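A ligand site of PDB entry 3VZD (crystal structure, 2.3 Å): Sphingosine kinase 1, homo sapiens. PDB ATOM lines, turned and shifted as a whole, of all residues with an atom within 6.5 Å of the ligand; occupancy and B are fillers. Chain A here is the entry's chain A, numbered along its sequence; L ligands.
The side-chain carboxylate (OD2) of Asp 175 is in hydrogen-bond range of an oxygen (O1) of the ligand (2.6 Å).
A nitrogen (N1) of the ligand sits at hydrogen-bond distance from the side-chain hydroxyl (OG1) of Thr 193 (3.0 Å).
The side-chain hydroxyl (OG1) of Thr 193 lies within hydrogen-bond range of the backbone carbonyl oxygen (O) of Phe 189 (2.8 Å).
O of Phe 285 is in hydrogen-bond range of N of Leu 258 (2.7 Å).
A ring nitrogen (NE2) of His 308 is in hydrogen-bond range of the backbone carbonyl oxygen (O) of Ala 271 (2.8 Å).
Merely in contact with the ligand: Phe 170 (3.5 Å), Ile 171 (3.6 Å), Val 174 (3.5 Å), Phe 189 (3.7 Å), Leu 265 (3.8 Å), Met 269 (3.6 Å), Phe 285 (3.1 Å), Leu 296 (3.3 Å), Phe 300 (3.4 Å), Met 303 (3.8 Å) and His 308 (3.7 Å).
Within 4 Å of the ligand: Phe 170, Ile 171, Val 174, Asp 175, Phe 189, Thr 193, Leu 265, Met 269, Phe 285, Leu 296, Phe 300, Met 303 and His 308.
The nearest printed residue that does not touch the ligand is Leu 256 (4.02 Å).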
ATOM      1  N   PHE A 170     -35.765 -25.431 -13.901  1.00  0.00           N
ATOM      2  CA  PHE A 170     -34.882 -24.504 -14.529  1.00  0.00           C
ATOM      3  C   PHE A 170     -34.816 -24.675 -16.059  1.00  0.00           C
ATOM      4  O   PHE A 170     -34.878 -23.689 -16.789  1.00  0.00           O
ATOM      5  CB  PHE A 170     -33.517 -24.727 -13.916  1.00  0.00           C
ATOM      6  CG  PHE A 170     -32.484 -23.756 -14.354  1.00  0.00           C
ATOM      7  CD1 PHE A 170     -31.829 -23.942 -15.554  1.00  0.00           C
ATOM      8  CD2 PHE A 170     -32.172 -22.647 -13.554  1.00  0.00           C
ATOM      9  CE1 PHE A 170     -30.803 -23.060 -15.963  1.00  0.00           C
ATOM     10  CE2 PHE A 170     -31.159 -21.768 -13.959  1.00  0.00           C
ATOM     11  CZ  PHE A 170     -30.464 -21.984 -15.192  1.00  0.00           C
ATOM     12  N   ILE A 171     -34.629 -25.907 -16.525  1.00  0.00           N
ATOM     13  CA  ILE A 171     -34.561 -26.171 -17.976  1.00  0.00           C
ATOM     14  C   ILE A 171     -35.840 -25.723 -18.709  1.00  0.00           C
ATOM     15  O   ILE A 171     -35.749 -25.086 -19.758  1.00  0.00           O
ATOM     16  CB  ILE A 171     -34.289 -27.632 -18.281  1.00  0.00           C
ATOM     17  CG1 ILE A 171     -32.848 -27.964 -17.950  1.00  0.00           C
ATOM     18  CG2 ILE A 171     -34.641 -27.997 -19.748  1.00  0.00           C
ATOM     19  CD1 ILE A 171     -32.611 -29.510 -18.083  1.00  0.00           C
ATOM     20  N   ALA A 172     -37.019 -26.015 -18.152  1.00  0.00           N
ATOM     21  CA  ALA A 172     -38.274 -25.600 -18.771  1.00  0.00           C
ATOM     22  C   ALA A 172     -38.486 -24.093 -18.766  1.00  0.00           C
ATOM     23  O   ALA A 172     -39.087 -23.531 -19.694  1.00  0.00           O
ATOM     24  CB  ALA A 172     -39.454 -26.258 -18.079  1.00  0.00           C
ATOM     25  N   VAL A 174     -36.135 -21.839 -18.872  1.00  0.00           N
ATOM     26  CA  VAL A 174     -35.247 -21.268 -19.836  1.00  0.00           C
ATOM     27  C   VAL A 174     -35.723 -21.558 -21.282  1.00  0.00           C
ATOM     28  O   VAL A 174     -35.618 -20.708 -22.118  1.00  0.00           O
ATOM     29  CB  VAL A 174     -33.788 -21.752 -19.566  1.00  0.00           C
ATOM     30  CG1 VAL A 174     -32.890 -21.531 -20.737  1.00  0.00           C
ATOM     31  CG2 VAL A 174     -33.262 -21.050 -18.353  1.00  0.00           C
ATOM     32  N   ASP A 175     -36.257 -22.745 -21.570  1.00  0.00           N
ATOM     33  CA  ASP A 175     -36.857 -22.978 -22.900  1.00  0.00           C
ATOM     34  C   ASP A 175     -37.906 -21.961 -23.151  1.00  0.00           C
ATOM     35  O   ASP A 175     -37.935 -21.374 -24.205  1.00  0.00           O
ATOM     36  CB  ASP A 175     -37.408 -24.386 -23.072  1.00  0.00           C
ATOM     37  CG  ASP A 175     -36.292 -25.405 -23.189  1.00  0.00           C
ATOM     38  OD1 ASP A 175     -36.540 -26.607 -23.353  1.00  0.00           O
ATOM     39  OD2 ASP A 175     -35.126 -24.960 -23.107  1.00  0.00           O
ATOM     40  N   PHE A 189     -29.702 -20.713 -25.261  1.00  0.00           N
ATOM     41  CA  PHE A 189     -29.876 -21.514 -24.070  1.00  0.00           C
ATOM     42  C   PHE A 189     -28.797 -21.172 -23.075  1.00  0.00           C
ATOM     43  O   PHE A 189     -29.043 -21.184 -21.904  1.00  0.00           O
ATOM     44  CB  PHE A 189     -29.948 -23.042 -24.371  1.00  0.00           C
ATOM     45  CG  PHE A 189     -31.088 -23.417 -25.239  1.00  0.00           C
ATOM     46  CD1 PHE A 189     -32.382 -23.321 -24.766  1.00  0.00           C
ATOM     47  CD2 PHE A 189     -30.867 -23.788 -26.564  1.00  0.00           C
ATOM     48  CE1 PHE A 189     -33.464 -23.624 -25.598  1.00  0.00           C
ATOM     49  CE2 PHE A 189     -31.937 -24.114 -27.417  1.00  0.00           C
ATOM     50  CZ  PHE A 189     -33.232 -24.029 -26.957  1.00  0.00           C
ATOM     51  N   GLY A 192     -29.911 -17.763 -21.831  1.00  0.00           N
ATOM     52  CA  GLY A 192     -31.038 -17.993 -20.943  1.00  0.00           C
ATOM     53  C   GLY A 192     -30.583 -18.583 -19.600  1.00  0.00           C
ATOM     54  O   GLY A 192     -31.089 -18.229 -18.525  1.00  0.00           O
ATOM     55  N   THR A 193     -29.636 -19.505 -19.661  1.00  0.00           N
ATOM     56  CA  THR A 193     -29.153 -20.185 -18.469  1.00  0.00           C
ATOM     57  C   THR A 193     -28.416 -19.171 -17.629  1.00  0.00           C
ATOM     58  O   THR A 193     -28.697 -19.036 -16.447  1.00  0.00           O
ATOM     59  CB  THR A 193     -28.260 -21.316 -18.891  1.00  0.00           C
ATOM     60  OG1 THR A 193     -29.108 -22.339 -19.403  1.00  0.00           O
ATOM     61  CG2 THR A 193     -27.430 -21.849 -17.731  1.00  0.00           C
ATOM     62  N   LEU A 197     -29.792 -18.090 -13.975  1.00  0.00           N
ATOM     63  CA  LEU A 197     -28.930 -18.353 -12.817  1.00  0.00           C
ATOM     64  C   LEU A 197     -28.935 -17.227 -11.777  1.00  0.00           C
ATOM     65  O   LEU A 197     -28.830 -17.504 -10.603  1.00  0.00           O
ATOM     66  CB  LEU A 197     -27.490 -18.668 -13.251  1.00  0.00           C
ATOM     67  CG  LEU A 197     -26.846 -20.048 -13.108  1.00  0.00           C
ATOM     68  CD1 LEU A 197     -27.777 -21.199 -12.834  1.00  0.00           C
ATOM     69  CD2 LEU A 197     -25.972 -20.420 -14.301  1.00  0.00           C
ATOM     70  N   LEU A 256     -34.105 -28.702 -11.170  1.00  0.00           N
ATOM     71  CA  LEU A 256     -34.626 -29.288 -12.428  1.00  0.00           C
ATOM     72  C   LEU A 256     -34.898 -30.789 -12.413  1.00  0.00           C
ATOM     73  O   LEU A 256     -34.233 -31.549 -11.748  1.00  0.00           O
ATOM     74  CB  LEU A 256     -33.693 -28.969 -13.593  1.00  0.00           C
ATOM     75  CG  LEU A 256     -32.352 -29.695 -13.587  1.00  0.00           C
ATOM     76  CD1 LEU A 256     -32.418 -31.104 -14.184  1.00  0.00           C
ATOM     77  CD2 LEU A 256     -31.286 -28.830 -14.345  1.00  0.00           C
ATOM     78  N   LEU A 258     -35.386 -33.839 -15.452  1.00  0.00           N
ATOM     79  CA  LEU A 258     -35.295 -34.090 -16.854  1.00  0.00           C
ATOM     80  C   LEU A 258     -35.447 -35.574 -17.136  1.00  0.00           C
ATOM     81  O   LEU A 258     -34.658 -36.398 -16.676  1.00  0.00           O
ATOM     82  CB  LEU A 258     -33.938 -33.565 -17.370  1.00  0.00           C
ATOM     83  CG  LEU A 258     -33.560 -33.860 -18.831  1.00  0.00           C
ATOM     84  CD1 LEU A 258     -34.593 -33.260 -19.808  1.00  0.00           C
ATOM     85  CD2 LEU A 258     -32.141 -33.336 -19.108  1.00  0.00           C
ATOM     86  N   LEU A 265     -29.324 -33.150 -25.442  1.00  0.00           N
ATOM     87  CA  LEU A 265     -30.335 -32.231 -25.027  1.00  0.00           C
ATOM     88  C   LEU A 265     -30.394 -31.073 -26.030  1.00  0.00           C
ATOM     89  O   LEU A 265     -31.353 -30.319 -26.041  1.00  0.00           O
ATOM     90  CB  LEU A 265     -29.957 -31.651 -23.702  1.00  0.00           C
ATOM     91  CG  LEU A 265     -30.865 -31.742 -22.522  1.00  0.00           C
ATOM     92  CD1 LEU A 265     -30.205 -30.796 -21.512  1.00  0.00           C
ATOM     93  CD2 LEU A 265     -32.429 -31.518 -22.836  1.00  0.00           C
ATOM     94  N   MET A 269     -24.922 -30.081 -26.393  1.00  0.00           N
ATOM     95  CA  MET A 269     -25.254 -30.482 -25.036  1.00  0.00           C
ATOM     96  C   MET A 269     -25.326 -32.020 -24.977  1.00  0.00           C
ATOM     97  O   MET A 269     -26.400 -32.586 -25.175  1.00  0.00           O
ATOM     98  CB  MET A 269     -26.600 -29.859 -24.666  1.00  0.00           C
ATOM     99  CG  MET A 269     -26.543 -28.365 -24.322  1.00  0.00           C
ATOM    100  SD  MET A 269     -28.134 -27.702 -23.714  1.00  0.00           S
ATOM    101  CE  MET A 269     -28.693 -26.842 -25.159  1.00  0.00           C
ATOM    102  N   ALA A 271     -25.757 -34.580 -23.008  1.00  0.00           N
ATOM    103  CA  ALA A 271     -26.247 -34.591 -21.618  1.00  0.00           C
ATOM    104  C   ALA A 271     -26.182 -36.016 -21.065  1.00  0.00           C
ATOM    105  O   ALA A 271     -26.079 -36.230 -19.878  1.00  0.00           O
ATOM    106  CB  ALA A 271     -27.665 -34.047 -21.520  1.00  0.00           C
ATOM    107  N   ALA A 272     -26.199 -36.993 -21.946  1.00  0.00           N
ATOM    108  CA  ALA A 272     -26.278 -38.352 -21.497  1.00  0.00           C
ATOM    109  C   ALA A 272     -25.191 -39.169 -22.131  1.00  0.00           C
ATOM    110  O   ALA A 272     -25.459 -39.952 -23.037  1.00  0.00           O
ATOM    111  CB  ALA A 272     -27.694 -38.952 -21.730  1.00  0.00           C
ATOM    112  N   PHE A 285     -32.756 -37.459 -14.858  1.00  0.00           N
ATOM    113  CA  PHE A 285     -31.838 -36.605 -14.167  1.00  0.00           C
ATOM    114  C   PHE A 285     -32.698 -35.709 -13.323  1.00  0.00           C
ATOM    115  O   PHE A 285     -33.784 -35.238 -13.757  1.00  0.00           O
ATOM    116  CB  PHE A 285     -31.068 -35.676 -15.155  1.00  0.00           C
ATOM    117  CG  PHE A 285     -30.114 -36.412 -16.091  1.00  0.00           C
ATOM    118  CD1 PHE A 285     -28.770 -36.546 -15.781  1.00  0.00           C
ATOM    119  CD2 PHE A 285     -30.575 -36.940 -17.317  1.00  0.00           C
ATOM    120  CE1 PHE A 285     -27.906 -37.190 -16.630  1.00  0.00           C
ATOM    121  CE2 PHE A 285     -29.720 -37.590 -18.176  1.00  0.00           C
ATOM    122  CZ  PHE A 285     -28.391 -37.736 -17.828  1.00  0.00           C
ATOM    123  N   VAL A 287     -31.789 -32.306 -10.305  1.00  0.00           N
ATOM    124  CA  VAL A 287     -30.873 -31.504  -9.525  1.00  0.00           C
ATOM    125  C   VAL A 287     -31.614 -31.059  -8.260  1.00  0.00           C
ATOM    126  O   VAL A 287     -32.640 -30.385  -8.337  1.00  0.00           O
ATOM    127  CB  VAL A 287     -30.306 -30.263 -10.335  1.00  0.00           C
ATOM    128  CG1 VAL A 287     -29.335 -29.418  -9.437  1.00  0.00           C
ATOM    129  CG2 VAL A 287     -29.519 -30.774 -11.576  1.00  0.00           C
ATOM    130  N   LEU A 296     -23.918 -25.233 -10.855  1.00  0.00           N
ATOM    131  CA  LEU A 296     -24.916 -25.392 -11.923  1.00  0.00           C
ATOM    132  C   LEU A 296     -24.354 -24.959 -13.322  1.00  0.00           C
ATOM    133  O   LEU A 296     -24.439 -25.727 -14.309  1.00  0.00           O
ATOM    134  CB  LEU A 296     -26.207 -24.650 -11.562  1.00  0.00           C
ATOM    135  CG  LEU A 296     -27.463 -25.433 -11.950  1.00  0.00           C
ATOM    136  CD1 LEU A 296     -28.425 -24.506 -12.616  1.00  0.00           C
ATOM    137  CD2 LEU A 296     -27.186 -26.627 -12.872  1.00  0.00           C
ATOM    138  N   LEU A 297     -23.695 -23.798 -13.363  1.00  0.00           N
ATOM    139  CA  LEU A 297     -23.024 -23.304 -14.597  1.00  0.00           C
ATOM    140  C   LEU A 297     -21.924 -24.192 -15.064  1.00  0.00           C
ATOM    141  O   LEU A 297     -21.850 -24.538 -16.270  1.00  0.00           O
ATOM    142  CB  LEU A 297     -22.518 -21.868 -14.467  1.00  0.00           C
ATOM    143  CG  LEU A 297     -21.902 -21.266 -15.722  1.00  0.00           C
ATOM    144  CD1 LEU A 297     -22.908 -21.137 -16.914  1.00  0.00           C
ATOM    145  CD2 LEU A 297     -21.371 -19.904 -15.375  1.00  0.00           C
ATOM    146  N   LEU A 299     -21.724 -27.299 -14.476  1.00  0.00           N
ATOM    147  CA  LEU A 299     -22.304 -28.556 -15.001  1.00  0.00           C
ATOM    148  C   LEU A 299     -22.838 -28.296 -16.445  1.00  0.00           C
ATOM    149  O   LEU A 299     -22.535 -29.023 -17.370  1.00  0.00           O
ATOM    150  CB  LEU A 299     -23.392 -29.136 -14.046  1.00  0.00           C
ATOM    151  CG  LEU A 299     -23.046 -29.708 -12.655  1.00  0.00           C
ATOM    152  CD1 LEU A 299     -24.326 -29.931 -11.781  1.00  0.00           C
ATOM    153  CD2 LEU A 299     -22.192 -30.976 -12.673  1.00  0.00           C
ATOM    154  N   PHE A 300     -23.582 -27.214 -16.597  1.00  0.00           N
ATOM    155  CA  PHE A 300     -23.988 -26.766 -17.933  1.00  0.00           C
ATOM    156  C   PHE A 300     -22.829 -26.737 -18.940  1.00  0.00           C
ATOM    157  O   PHE A 300     -22.871 -27.451 -19.945  1.00  0.00           O
ATOM    158  CB  PHE A 300     -24.563 -25.394 -17.864  1.00  0.00           C
ATOM    159  CG  PHE A 300     -25.112 -24.909 -19.190  1.00  0.00           C
ATOM    160  CD1 PHE A 300     -26.282 -25.457 -19.708  1.00  0.00           C
ATOM    161  CD2 PHE A 300     -24.482 -23.874 -19.882  1.00  0.00           C
ATOM    162  CE1 PHE A 300     -26.797 -25.022 -20.905  1.00  0.00           C
ATOM    163  CE2 PHE A 300     -24.993 -23.393 -21.081  1.00  0.00           C
ATOM    164  CZ  PHE A 300     -26.160 -23.955 -21.603  1.00  0.00           C
ATOM    165  N   MET A 303     -21.267 -29.821 -20.167  1.00  0.00           N
ATOM    166  CA  MET A 303     -22.209 -30.628 -20.938  1.00  0.00           C
ATOM    167  C   MET A 303     -21.919 -30.634 -22.426  1.00  0.00           C
ATOM    168  O   MET A 303     -22.123 -31.639 -23.117  1.00  0.00           O
ATOM    169  CB  MET A 303     -23.644 -30.203 -20.616  1.00  0.00           C
ATOM    170  CG  MET A 303     -24.692 -30.949 -21.366  1.00  0.00           C
ATOM    171  SD  MET A 303     -26.209 -30.765 -20.479  1.00  0.00           S
ATOM    172  CE  MET A 303     -26.412 -29.003 -20.228  1.00  0.00           C
ATOM    173  N   HIS A 308     -20.012 -33.469 -17.602  1.00  0.00           N
ATOM    174  CA  HIS A 308     -20.644 -32.993 -16.376  1.00  0.00           C
ATOM    175  C   HIS A 308     -20.777 -34.087 -15.315  1.00  0.00           C
ATOM    176  O   HIS A 308     -20.877 -33.774 -14.137  1.00  0.00           O
ATOM    177  CB  HIS A 308     -22.008 -32.373 -16.701  1.00  0.00           C
ATOM    178  CG  HIS A 308     -22.886 -33.287 -17.486  1.00  0.00           C
ATOM    179  ND1 HIS A 308     -22.567 -33.709 -18.763  1.00  0.00           N
ATOM    180  CD2 HIS A 308     -24.055 -33.895 -17.183  1.00  0.00           C
ATOM    181  CE1 HIS A 308     -23.527 -34.494 -19.226  1.00  0.00           C
ATOM    182  NE2 HIS A 308     -24.431 -34.630 -18.277  1.00  0.00           N
ATOM    183  N   MET A 309     -20.763 -35.355 -15.730  1.00  0.00           N
ATOM    184  CA  MET A 309     -20.902 -36.515 -14.789  1.00  0.00           C
ATOM    185  C   MET A 309     -19.633 -36.717 -13.958  1.00  0.00           C
ATOM    186  O   MET A 309     -19.658 -37.325 -12.876  1.00  0.00           O
ATOM    187  CB  MET A 309     -21.266 -37.838 -15.524  1.00  0.00           C
ATOM    188  CG  MET A 309     -22.684 -37.876 -16.212  1.00  0.00           C
ATOM    189  SD  MET A 309     -24.041 -37.061 -15.327  1.00  0.00           S
ATOM    190  CE  MET A 309     -24.463 -38.360 -14.126  1.00  0.00           C
ATOM    191  N   LEU A 316     -26.685 -33.707  -8.164  1.00  0.00           N
ATOM    192  CA  LEU A 316     -27.218 -34.141  -9.451  1.00  0.00           C
ATOM    193  C   LEU A 316     -27.366 -35.617  -9.416  1.00  0.00           C
ATOM    194  O   LEU A 316     -26.363 -36.341  -9.241  1.00  0.00           O
ATOM    195  CB  LEU A 316     -26.261 -33.754 -10.612  1.00  0.00           C
ATOM    196  CG  LEU A 316     -26.487 -34.420 -12.016  1.00  0.00           C
ATOM    197  CD1 LEU A 316     -27.850 -33.974 -12.727  1.00  0.00           C
ATOM    198  CD2 LEU A 316     -25.242 -34.349 -12.972  1.00  0.00           C
HETATM  199  C1  LIG L   1     -30.292 -26.746 -20.627  1.00  0.00           C
HETATM  200  C2  LIG L   1     -31.093 -27.079 -21.721  1.00  0.00           C
HETATM  201  C3  LIG L   1     -32.167 -26.230 -22.018  1.00  0.00           C
HETATM  202  O1  LIG L   1     -33.025 -26.505 -23.023  1.00  0.00           O
HETATM  203  C4  LIG L   1     -32.439 -25.099 -21.253  1.00  0.00           C
HETATM  204  C5  LIG L   1     -31.633 -24.783 -20.176  1.00  0.00           C
HETATM  205  C6  LIG L   1     -30.548 -25.590 -19.864  1.00  0.00           C
HETATM  206  N1  LIG L   1     -29.822 -25.194 -18.793  1.00  0.00           N
HETATM  207  C7  LIG L   1     -29.174 -26.001 -17.922  1.00  0.00           C
HETATM  208  N2  LIG L   1     -29.086 -27.352 -17.967  1.00  0.00           N
HETATM  209  S1  LIG L   1     -28.256 -25.437 -16.577  1.00  0.00           S
HETATM  210  C8  LIG L   1     -27.749 -27.016 -16.123  1.00  0.00           C
HETATM  211  C9  LIG L   1     -28.350 -27.917 -16.962  1.00  0.00           C
HETATM  212  C10 LIG L   1     -28.194 -29.293 -16.874  1.00  0.00           C
HETATM  213  C11 LIG L   1     -28.991 -30.107 -17.694  1.00  0.00           C
HETATM  214  C12 LIG L   1     -28.859 -31.486 -17.696  1.00  0.00           C
HETATM  215  C13 LIG L   1     -27.929 -32.085 -16.831  1.00  0.00           C
HETATM  216 CL1  LIG L   1     -27.788 -33.810 -16.829  1.00  0.00          CL
HETATM  217  C14 LIG L   1     -27.148 -31.273 -16.016  1.00  0.00           C
HETATM  218  C15 LIG L   1     -27.254 -29.888 -16.023  1.00  0.00           C
